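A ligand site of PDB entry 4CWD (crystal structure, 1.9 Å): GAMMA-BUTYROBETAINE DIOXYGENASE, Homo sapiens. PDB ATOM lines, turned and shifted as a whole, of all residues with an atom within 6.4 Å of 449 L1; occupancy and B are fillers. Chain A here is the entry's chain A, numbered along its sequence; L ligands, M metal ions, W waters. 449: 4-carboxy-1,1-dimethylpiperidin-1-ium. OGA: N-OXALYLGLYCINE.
The backbone NH (N) of Tyr 206 is in hydrogen-bond range of an oxygen (OAI) of 449 L1 (2.7 Å).
An oxygen (OAI) of 449 L1 lies within hydrogen-bond range of the side-chain amide nitrogen (ND2) of Asn 293, 3.0 Å away.
An oxygen (OAJ) of 449 L1 lies within hydrogen-bond range of the side-chain amide nitrogen (ND2) of Asn 192, at 3.0 Å.
Residues that only touch 449 L1: Trp 182 (3.3 Å), Tyr 367 (3.3 Å), Tyr 195 (3.4 Å), Thr 296 (3.5 Å), Asp 205 (3.5 Å), Tyr 178 (3.5 Å) and Pro 207 (3.7 Å).
The nearest printed residue that does not touch 449 L1 is Ala 194 (4.3 Å).
Water W1 lies within hydrogen-bond range of OD1 of Asn 192, OAJ of 449 L1 and ND2 of Asn 293.
Water W3 bridges OAJ of 449 L1 and OD2 of Asp 262.
Water W2 lies within hydrogen-bond range of an oxygen (OAI) of 449 L1 (2.8 Å), the side-chain hydroxyl of Thr 296 (2.9 Å) and the backbone NH of Ala 208 (3.1 Å).
OD1 of Asn 293 is in hydrogen-bond range of N of Ala 295, at 3.0 Å.
OD2 of Asp 205 sits at hydrogen-bond distance from NE2 of Gln 216 (3.2 Å).
OD2 of Asp 205 is in hydrogen-bond range of OH of Tyr 367.
The side-chain hydroxyl (OG1) of Thr 176 lies close to the backbone NH (N) of Tyr 178, at 3.3 Å.
OD1 of Asn 192 sits at hydrogen-bond distance from N of Ala 194 (3.0 Å).
The backbone carbonyl oxygen (O) of Asn 293 sits at hydrogen-bond distance from the side-chain hydroxyl (OG1) of Thr 296, at 3.5 Å.
The side-chain carboxylate of Asp 262 sits at hydrogen-bond distance from the side-chain hydroxyl of Tyr 178 (2.7 Å).
The side-chain amide nitrogen of Asn 192 sits at hydrogen-bond distance from the side-chain hydroxyl of Tyr 178.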
ATOM      1  N   THR A 176      12.065 -16.654  11.763  1.00  0.00           N
ATOM      2  CA  THR A 176      11.128 -17.641  11.230  1.00  0.00           C
ATOM      3  C   THR A 176      10.691 -18.563  12.358  1.00  0.00           C
ATOM      4  O   THR A 176      11.165 -18.436  13.482  1.00  0.00           O
ATOM      5  CB  THR A 176      11.740 -18.494  10.086  1.00  0.00           C
ATOM      6  OG1 THR A 176      12.677 -19.437  10.620  1.00  0.00           O
ATOM      7  CG2 THR A 176      12.431 -17.615   9.036  1.00  0.00           C
ATOM      8  N   TYR A 178      11.585 -21.387  13.040  1.00  0.00           N
ATOM      9  CA  TYR A 178      12.683 -22.195  13.562  1.00  0.00           C
ATOM     10  C   TYR A 178      13.647 -21.387  14.433  1.00  0.00           C
ATOM     11  O   TYR A 178      14.639 -21.915  14.926  1.00  0.00           O
ATOM     12  CB  TYR A 178      13.436 -22.879  12.412  1.00  0.00           C
ATOM     13  CG  TYR A 178      12.621 -23.991  11.777  1.00  0.00           C
ATOM     14  CD1 TYR A 178      12.618 -25.261  12.326  1.00  0.00           C
ATOM     15  CD2 TYR A 178      11.847 -23.757  10.644  1.00  0.00           C
ATOM     16  CE1 TYR A 178      11.873 -26.280  11.762  1.00  0.00           C
ATOM     17  CE2 TYR A 178      11.097 -24.768  10.081  1.00  0.00           C
ATOM     18  CZ  TYR A 178      11.120 -26.023  10.637  1.00  0.00           C
ATOM     19  OH  TYR A 178      10.374 -27.044  10.082  1.00  0.00           O
ATOM     20  N   TRP A 182      19.298 -21.215  14.387  1.00  0.00           N
ATOM     21  CA  TRP A 182      18.864 -22.595  14.564  1.00  0.00           C
ATOM     22  C   TRP A 182      20.042 -23.543  14.409  1.00  0.00           C
ATOM     23  O   TRP A 182      21.026 -23.237  13.724  1.00  0.00           O
ATOM     24  CB  TRP A 182      17.755 -22.947  13.561  1.00  0.00           C
ATOM     25  CG  TRP A 182      17.782 -22.117  12.305  1.00  0.00           C
ATOM     26  CD1 TRP A 182      17.101 -20.939  12.083  1.00  0.00           C
ATOM     27  CD2 TRP A 182      18.500 -22.393  11.111  1.00  0.00           C
ATOM     28  NE1 TRP A 182      17.368 -20.479  10.814  1.00  0.00           N
ATOM     29  CE2 TRP A 182      18.231 -21.350  10.198  1.00  0.00           C
ATOM     30  CE3 TRP A 182      19.366 -23.430  10.718  1.00  0.00           C
ATOM     31  CZ2 TRP A 182      18.785 -21.303   8.924  1.00  0.00           C
ATOM     32  CZ3 TRP A 182      19.905 -23.383   9.453  1.00  0.00           C
ATOM     33  CH2 TRP A 182      19.622 -22.328   8.570  1.00  0.00           C
ATOM     34  N   VAL A 184      21.644 -26.985  13.287  1.00  0.00           N
ATOM     35  CA  VAL A 184      21.552 -28.093  12.363  1.00  0.00           C
ATOM     36  C   VAL A 184      22.343 -29.237  12.948  1.00  0.00           C
ATOM     37  O   VAL A 184      23.571 -29.248  12.891  1.00  0.00           O
ATOM     38  CB  VAL A 184      22.065 -27.715  10.968  1.00  0.00           C
ATOM     39  CG1 VAL A 184      21.863 -28.871   9.987  1.00  0.00           C
ATOM     40  CG2 VAL A 184      21.358 -26.449  10.472  1.00  0.00           C
ATOM     41  N   ASN A 191      11.812 -32.385  13.739  1.00  0.00           N
ATOM     42  CA  ASN A 191      10.672 -31.709  13.122  1.00  0.00           C
ATOM     43  C   ASN A 191      10.980 -31.286  11.686  1.00  0.00           C
ATOM     44  O   ASN A 191      10.184 -30.620  11.043  1.00  0.00           O
ATOM     45  CB  ASN A 191      10.230 -30.504  13.971  1.00  0.00           C
ATOM     46  CG  ASN A 191      11.293 -29.408  14.050  1.00  0.00           C
ATOM     47  OD1 ASN A 191      12.242 -29.373  13.283  1.00  0.00           O
ATOM     48  ND2 ASN A 191      11.077 -28.464  14.969  1.00  0.00           N
ATOM     49  N   ASN A 192      12.153 -31.691  11.210  1.00  0.00           N
ATOM     50  CA  ASN A 192      12.623 -31.289   9.885  1.00  0.00           C
ATOM     51  C   ASN A 192      13.722 -32.237   9.440  1.00  0.00           C
ATOM     52  O   ASN A 192      14.564 -32.624  10.241  1.00  0.00           O
ATOM     53  CB  ASN A 192      13.135 -29.852   9.916  1.00  0.00           C
ATOM     54  CG  ASN A 192      13.256 -29.232   8.536  1.00  0.00           C
ATOM     55  OD1 ASN A 192      14.181 -29.554   7.785  1.00  0.00           O
ATOM     56  ND2 ASN A 192      12.341 -28.336   8.203  1.00  0.00           N
ATOM     57  N   VAL A 193      13.731 -32.616   8.156  1.00  0.00           N
ATOM     58  CA  VAL A 193      14.740 -33.580   7.685  1.00  0.00           C
ATOM     59  C   VAL A 193      16.162 -33.016   7.837  1.00  0.00           C
ATOM     60  O   VAL A 193      17.133 -33.763   7.900  1.00  0.00           O
ATOM     61  CB  VAL A 193      14.517 -34.005   6.214  1.00  0.00           C
ATOM     62  CG1 VAL A 193      13.182 -34.739   6.059  1.00  0.00           C
ATOM     63  CG2 VAL A 193      14.602 -32.802   5.270  1.00  0.00           C
ATOM     64  N   ALA A 194      16.280 -31.694   7.913  1.00  0.00           N
ATOM     65  CA  ALA A 194      17.582 -31.070   8.123  1.00  0.00           C
ATOM     66  C   ALA A 194      18.190 -31.499   9.459  1.00  0.00           C
ATOM     67  O   ALA A 194      19.409 -31.565   9.606  1.00  0.00           O
ATOM     68  CB  ALA A 194      17.450 -29.541   8.062  1.00  0.00           C
ATOM     69  N   TYR A 195      17.326 -31.790  10.422  1.00  0.00           N
ATOM     70  CA  TYR A 195      17.778 -32.116  11.768  1.00  0.00           C
ATOM     71  C   TYR A 195      17.903 -33.645  11.900  1.00  0.00           C
ATOM     72  O   TYR A 195      17.539 -34.216  12.926  1.00  0.00           O
ATOM     73  CB  TYR A 195      16.817 -31.533  12.806  1.00  0.00           C
ATOM     74  CG  TYR A 195      16.668 -30.017  12.750  1.00  0.00           C
ATOM     75  CD1 TYR A 195      17.676 -29.209  12.225  1.00  0.00           C
ATOM     76  CD2 TYR A 195      15.525 -29.383  13.237  1.00  0.00           C
ATOM     77  CE1 TYR A 195      17.543 -27.825  12.175  1.00  0.00           C
ATOM     78  CE2 TYR A 195      15.386 -27.990  13.188  1.00  0.00           C
ATOM     79  CZ  TYR A 195      16.400 -27.215  12.667  1.00  0.00           C
ATOM     80  OH  TYR A 195      16.262 -25.846  12.624  1.00  0.00           O
ATOM     81  N   HIS A 203      18.323 -28.168  -2.727  1.00  0.00           N
ATOM     82  CA  HIS A 203      17.104 -27.488  -2.324  1.00  0.00           C
ATOM     83  C   HIS A 203      17.413 -26.034  -1.998  1.00  0.00           C
ATOM     84  O   HIS A 203      18.555 -25.664  -1.750  1.00  0.00           O
ATOM     85  CB  HIS A 203      16.472 -28.175  -1.102  1.00  0.00           C
ATOM     86  CG  HIS A 203      17.302 -28.082   0.137  1.00  0.00           C
ATOM     87  ND1 HIS A 203      18.395 -28.893   0.370  1.00  0.00           N
ATOM     88  CD2 HIS A 203      17.195 -27.280   1.228  1.00  0.00           C
ATOM     89  CE1 HIS A 203      18.921 -28.587   1.538  1.00  0.00           C
ATOM     90  NE2 HIS A 203      18.207 -27.617   2.083  1.00  0.00           N
ATOM     91  N   THR A 204      16.370 -25.217  -2.026  1.00  0.00           N
ATOM     92  CA  THR A 204      16.396 -23.900  -1.408  1.00  0.00           C
ATOM     93  C   THR A 204      15.726 -24.051  -0.049  1.00  0.00           C
ATOM     94  O   THR A 204      14.890 -24.932   0.114  1.00  0.00           O
ATOM     95  CB  THR A 204      15.641 -22.844  -2.253  1.00  0.00           C
ATOM     96  OG1 THR A 204      14.259 -23.221  -2.382  1.00  0.00           O
ATOM     97  CG2 THR A 204      16.258 -22.734  -3.638  1.00  0.00           C
ATOM     98  N   ASP A 205      16.090 -23.206   0.910  1.00  0.00           N
ATOM     99  CA  ASP A 205      15.422 -23.231   2.214  1.00  0.00           C
ATOM    100  C   ASP A 205      14.097 -22.496   2.222  1.00  0.00           C
ATOM    101  O   ASP A 205      13.979 -21.406   1.669  1.00  0.00           O
ATOM    102  CB  ASP A 205      16.310 -22.636   3.298  1.00  0.00           C
ATOM    103  CG  ASP A 205      17.166 -23.678   3.954  1.00  0.00           C
ATOM    104  OD1 ASP A 205      17.339 -24.704   3.290  1.00  0.00           O
ATOM    105  OD2 ASP A 205      17.629 -23.478   5.092  1.00  0.00           O
ATOM    106  N   TYR A 206      13.132 -23.119   2.895  1.00  0.00           N
ATOM    107  CA  TYR A 206      11.861 -22.503   3.277  1.00  0.00           C
ATOM    108  C   TYR A 206      10.956 -22.052   2.120  1.00  0.00           C
ATOM    109  O   TYR A 206      10.374 -20.966   2.182  1.00  0.00           O
ATOM    110  CB  TYR A 206      12.144 -21.330   4.232  1.00  0.00           C
ATOM    111  CG  TYR A 206      11.477 -21.467   5.594  1.00  0.00           C
ATOM    112  CD1 TYR A 206      10.230 -22.054   5.730  1.00  0.00           C
ATOM    113  CD2 TYR A 206      12.120 -21.006   6.739  1.00  0.00           C
ATOM    114  CE1 TYR A 206       9.626 -22.163   6.973  1.00  0.00           C
ATOM    115  CE2 TYR A 206      11.523 -21.109   7.985  1.00  0.00           C
ATOM    116  CZ  TYR A 206      10.275 -21.682   8.092  1.00  0.00           C
ATOM    117  OH  TYR A 206       9.690 -21.776   9.320  1.00  0.00           O
ATOM    118  N   PRO A 207      10.797 -22.894   1.097  1.00  0.00           N
ATOM    119  CA  PRO A 207       9.764 -22.566   0.113  1.00  0.00           C
ATOM    120  C   PRO A 207       8.353 -22.661   0.699  1.00  0.00           C
ATOM    121  O   PRO A 207       7.413 -22.234   0.048  1.00  0.00           O
ATOM    122  CB  PRO A 207       9.968 -23.614  -0.984  1.00  0.00           C
ATOM    123  CG  PRO A 207      10.626 -24.773  -0.267  1.00  0.00           C
ATOM    124  CD  PRO A 207      11.540 -24.115   0.721  1.00  0.00           C
ATOM    125  N   ALA A 208       8.220 -23.218   1.895  1.00  0.00           N
ATOM    126  CA  ALA A 208       6.909 -23.263   2.577  1.00  0.00           C
ATOM    127  C   ALA A 208       6.431 -21.857   2.937  1.00  0.00           C
ATOM    128  O   ALA A 208       5.284 -21.668   3.289  1.00  0.00           O
ATOM    129  CB  ALA A 208       6.975 -24.139   3.806  1.00  0.00           C
ATOM    130  N   GLN A 216      21.139 -16.901   3.326  1.00  0.00           N
ATOM    131  CA  GLN A 216      21.299 -17.897   4.368  1.00  0.00           C
ATOM    132  C   GLN A 216      22.705 -17.849   4.905  1.00  0.00           C
ATOM    133  O   GLN A 216      23.670 -17.664   4.152  1.00  0.00           O
ATOM    134  CB  GLN A 216      20.975 -19.287   3.826  1.00  0.00           C
ATOM    135  CG  GLN A 216      21.044 -20.374   4.878  1.00  0.00           C
ATOM    136  CD  GLN A 216      20.637 -21.735   4.362  1.00  0.00           C
ATOM    137  OE1 GLN A 216      21.101 -22.752   4.875  1.00  0.00           O
ATOM    138  NE2 GLN A 216      19.763 -21.779   3.364  1.00  0.00           N
ATOM    139  N   ASP A 262       4.595 -27.140   5.909  1.00  0.00           N
ATOM    140  CA  ASP A 262       5.463 -27.367   7.077  1.00  0.00           C
ATOM    141  C   ASP A 262       4.635 -27.260   8.333  1.00  0.00           C
ATOM    142  O   ASP A 262       4.097 -26.203   8.653  1.00  0.00           O
ATOM    143  CB  ASP A 262       6.622 -26.370   7.097  1.00  0.00           C
ATOM    144  CG  ASP A 262       7.780 -26.803   8.015  1.00  0.00           C
ATOM    145  OD1 ASP A 262       7.917 -28.015   8.308  1.00  0.00           O
ATOM    146  OD2 ASP A 262       8.582 -25.927   8.403  1.00  0.00           O
ATOM    147  N   ASN A 293      12.195 -27.351  -2.357  1.00  0.00           N
ATOM    148  CA  ASN A 293      12.705 -28.259  -1.350  1.00  0.00           C
ATOM    149  C   ASN A 293      11.869 -29.537  -1.404  1.00  0.00           C
ATOM    150  O   ASN A 293      10.670 -29.489  -1.130  1.00  0.00           O
ATOM    151  CB  ASN A 293      12.652 -27.627   0.042  1.00  0.00           C
ATOM    152  CG  ASN A 293      13.353 -28.460   1.101  1.00  0.00           C
ATOM    153  OD1 ASN A 293      13.457 -29.677   0.986  1.00  0.00           O
ATOM    154  ND2 ASN A 293      13.850 -27.803   2.143  1.00  0.00           N
ATOM    155  N   ALA A 295      11.673 -32.010   0.414  1.00  0.00           N
ATOM    156  CA  ALA A 295      11.202 -32.489   1.692  1.00  0.00           C
ATOM    157  C   ALA A 295       9.863 -31.879   2.074  1.00  0.00           C
ATOM    158  O   ALA A 295       9.024 -32.547   2.683  1.00  0.00           O
ATOM    159  CB  ALA A 295      12.244 -32.200   2.775  1.00  0.00           C
ATOM    160  N   THR A 296       9.666 -30.613   1.712  1.00  0.00           N
ATOM    161  CA  THR A 296       8.485 -29.865   2.135  1.00  0.00           C
ATOM    162  C   THR A 296       7.462 -29.679   1.019  1.00  0.00           C
ATOM    163  O   THR A 296       6.348 -29.186   1.254  1.00  0.00           O
ATOM    164  CB  THR A 296       8.893 -28.485   2.696  1.00  0.00           C
ATOM    165  OG1 THR A 296       9.554 -27.734   1.677  1.00  0.00           O
ATOM    166  CG2 THR A 296       9.827 -28.652   3.886  1.00  0.00           C
ATOM    167  N   TYR A 367      18.911 -16.574   8.793  1.00  0.00           N
ATOM    168  CA  TYR A 367      18.456 -16.013   7.526  1.00  0.00           C
ATOM    169  C   TYR A 367      18.512 -14.490   7.573  1.00  0.00           C
ATOM    170  O   TYR A 367      18.468 -13.897   8.659  1.00  0.00           O
ATOM    171  CB  TYR A 367      17.017 -16.439   7.225  1.00  0.00           C
ATOM    172  CG  TYR A 367      16.814 -17.942   7.058  1.00  0.00           C
ATOM    173  CD1 TYR A 367      17.495 -18.645   6.090  1.00  0.00           C
ATOM    174  CD2 TYR A 367      15.898 -18.620   7.850  1.00  0.00           C
ATOM    175  CE1 TYR A 367      17.294 -20.006   5.922  1.00  0.00           C
ATOM    176  CE2 TYR A 367      15.699 -19.970   7.696  1.00  0.00           C
ATOM    177  CZ  TYR A 367      16.390 -20.657   6.742  1.00  0.00           C
ATOM    178  OH  TYR A 367      16.192 -22.004   6.578  1.00  0.00           O
HETATM  179  CAA 449 L   1      13.414 -24.777   7.249  1.00  0.00           C
HETATM  180  CAB 449 L   1      14.395 -24.187   8.263  1.00  0.00           C
HETATM  181  CAC 449 L   1      16.052 -25.579   7.391  1.00  0.00           C
HETATM  182  CAD 449 L   1      15.136 -26.174   6.458  1.00  0.00           C
HETATM  183  CAE 449 L   1      14.009 -25.278   5.940  1.00  0.00           C
HETATM  184  CAF 449 L   1      16.474 -24.295   9.378  1.00  0.00           C
HETATM  185  CAG 449 L   1      15.031 -26.159   9.457  1.00  0.00           C
HETATM  186  CAH 449 L   1      12.979 -26.000   5.088  1.00  0.00           C
HETATM  187  OAI 449 L   1      12.781 -25.633   3.899  1.00  0.00           O
HETATM  188  OAJ 449 L   1      12.331 -26.949   5.583  1.00  0.00           O
HETATM  189  NAK 449 L   1      15.498 -25.055   8.629  1.00  0.00           N
HETATM  190  C1  OGA L   2      19.265 -27.276   6.077  1.00  0.00           C
HETATM  191  C2  OGA L   2      20.582 -27.519   5.376  1.00  0.00           C
HETATM  192  C4  OGA L   2      22.850 -28.303   5.264  1.00  0.00           C
HETATM  193  C5  OGA L   2      23.810 -29.124   6.073  1.00  0.00           C
HETATM  194  O1  OGA L   2      19.254 -27.058   7.317  1.00  0.00           O
HETATM  195  O2  OGA L   2      18.173 -27.284   5.427  1.00  0.00           O
HETATM  196  O2' OGA L   2      20.778 -27.176   4.228  1.00  0.00           O
HETATM  197  O3  OGA L   2      23.368 -29.784   7.049  1.00  0.00           O
HETATM  198  N1  OGA L   2      21.661 -28.142   6.017  1.00  0.00           N
HETATM  199  O4  OGA L   2      25.016 -29.139   5.745  1.00  0.00           O
HETATM  200 NI    NI M   1      18.971 -26.082   3.521  1.00  0.00          NI
HETATM  201  O   HOH W   1      13.466 -29.375   5.185  1.00  0.00           O
HETATM  202  O   HOH W   2      10.073 -25.324   3.211  1.00  0.00           O
HETATM  203  O   HOH W   3       9.951 -25.570   5.855  1.00  0.00           O
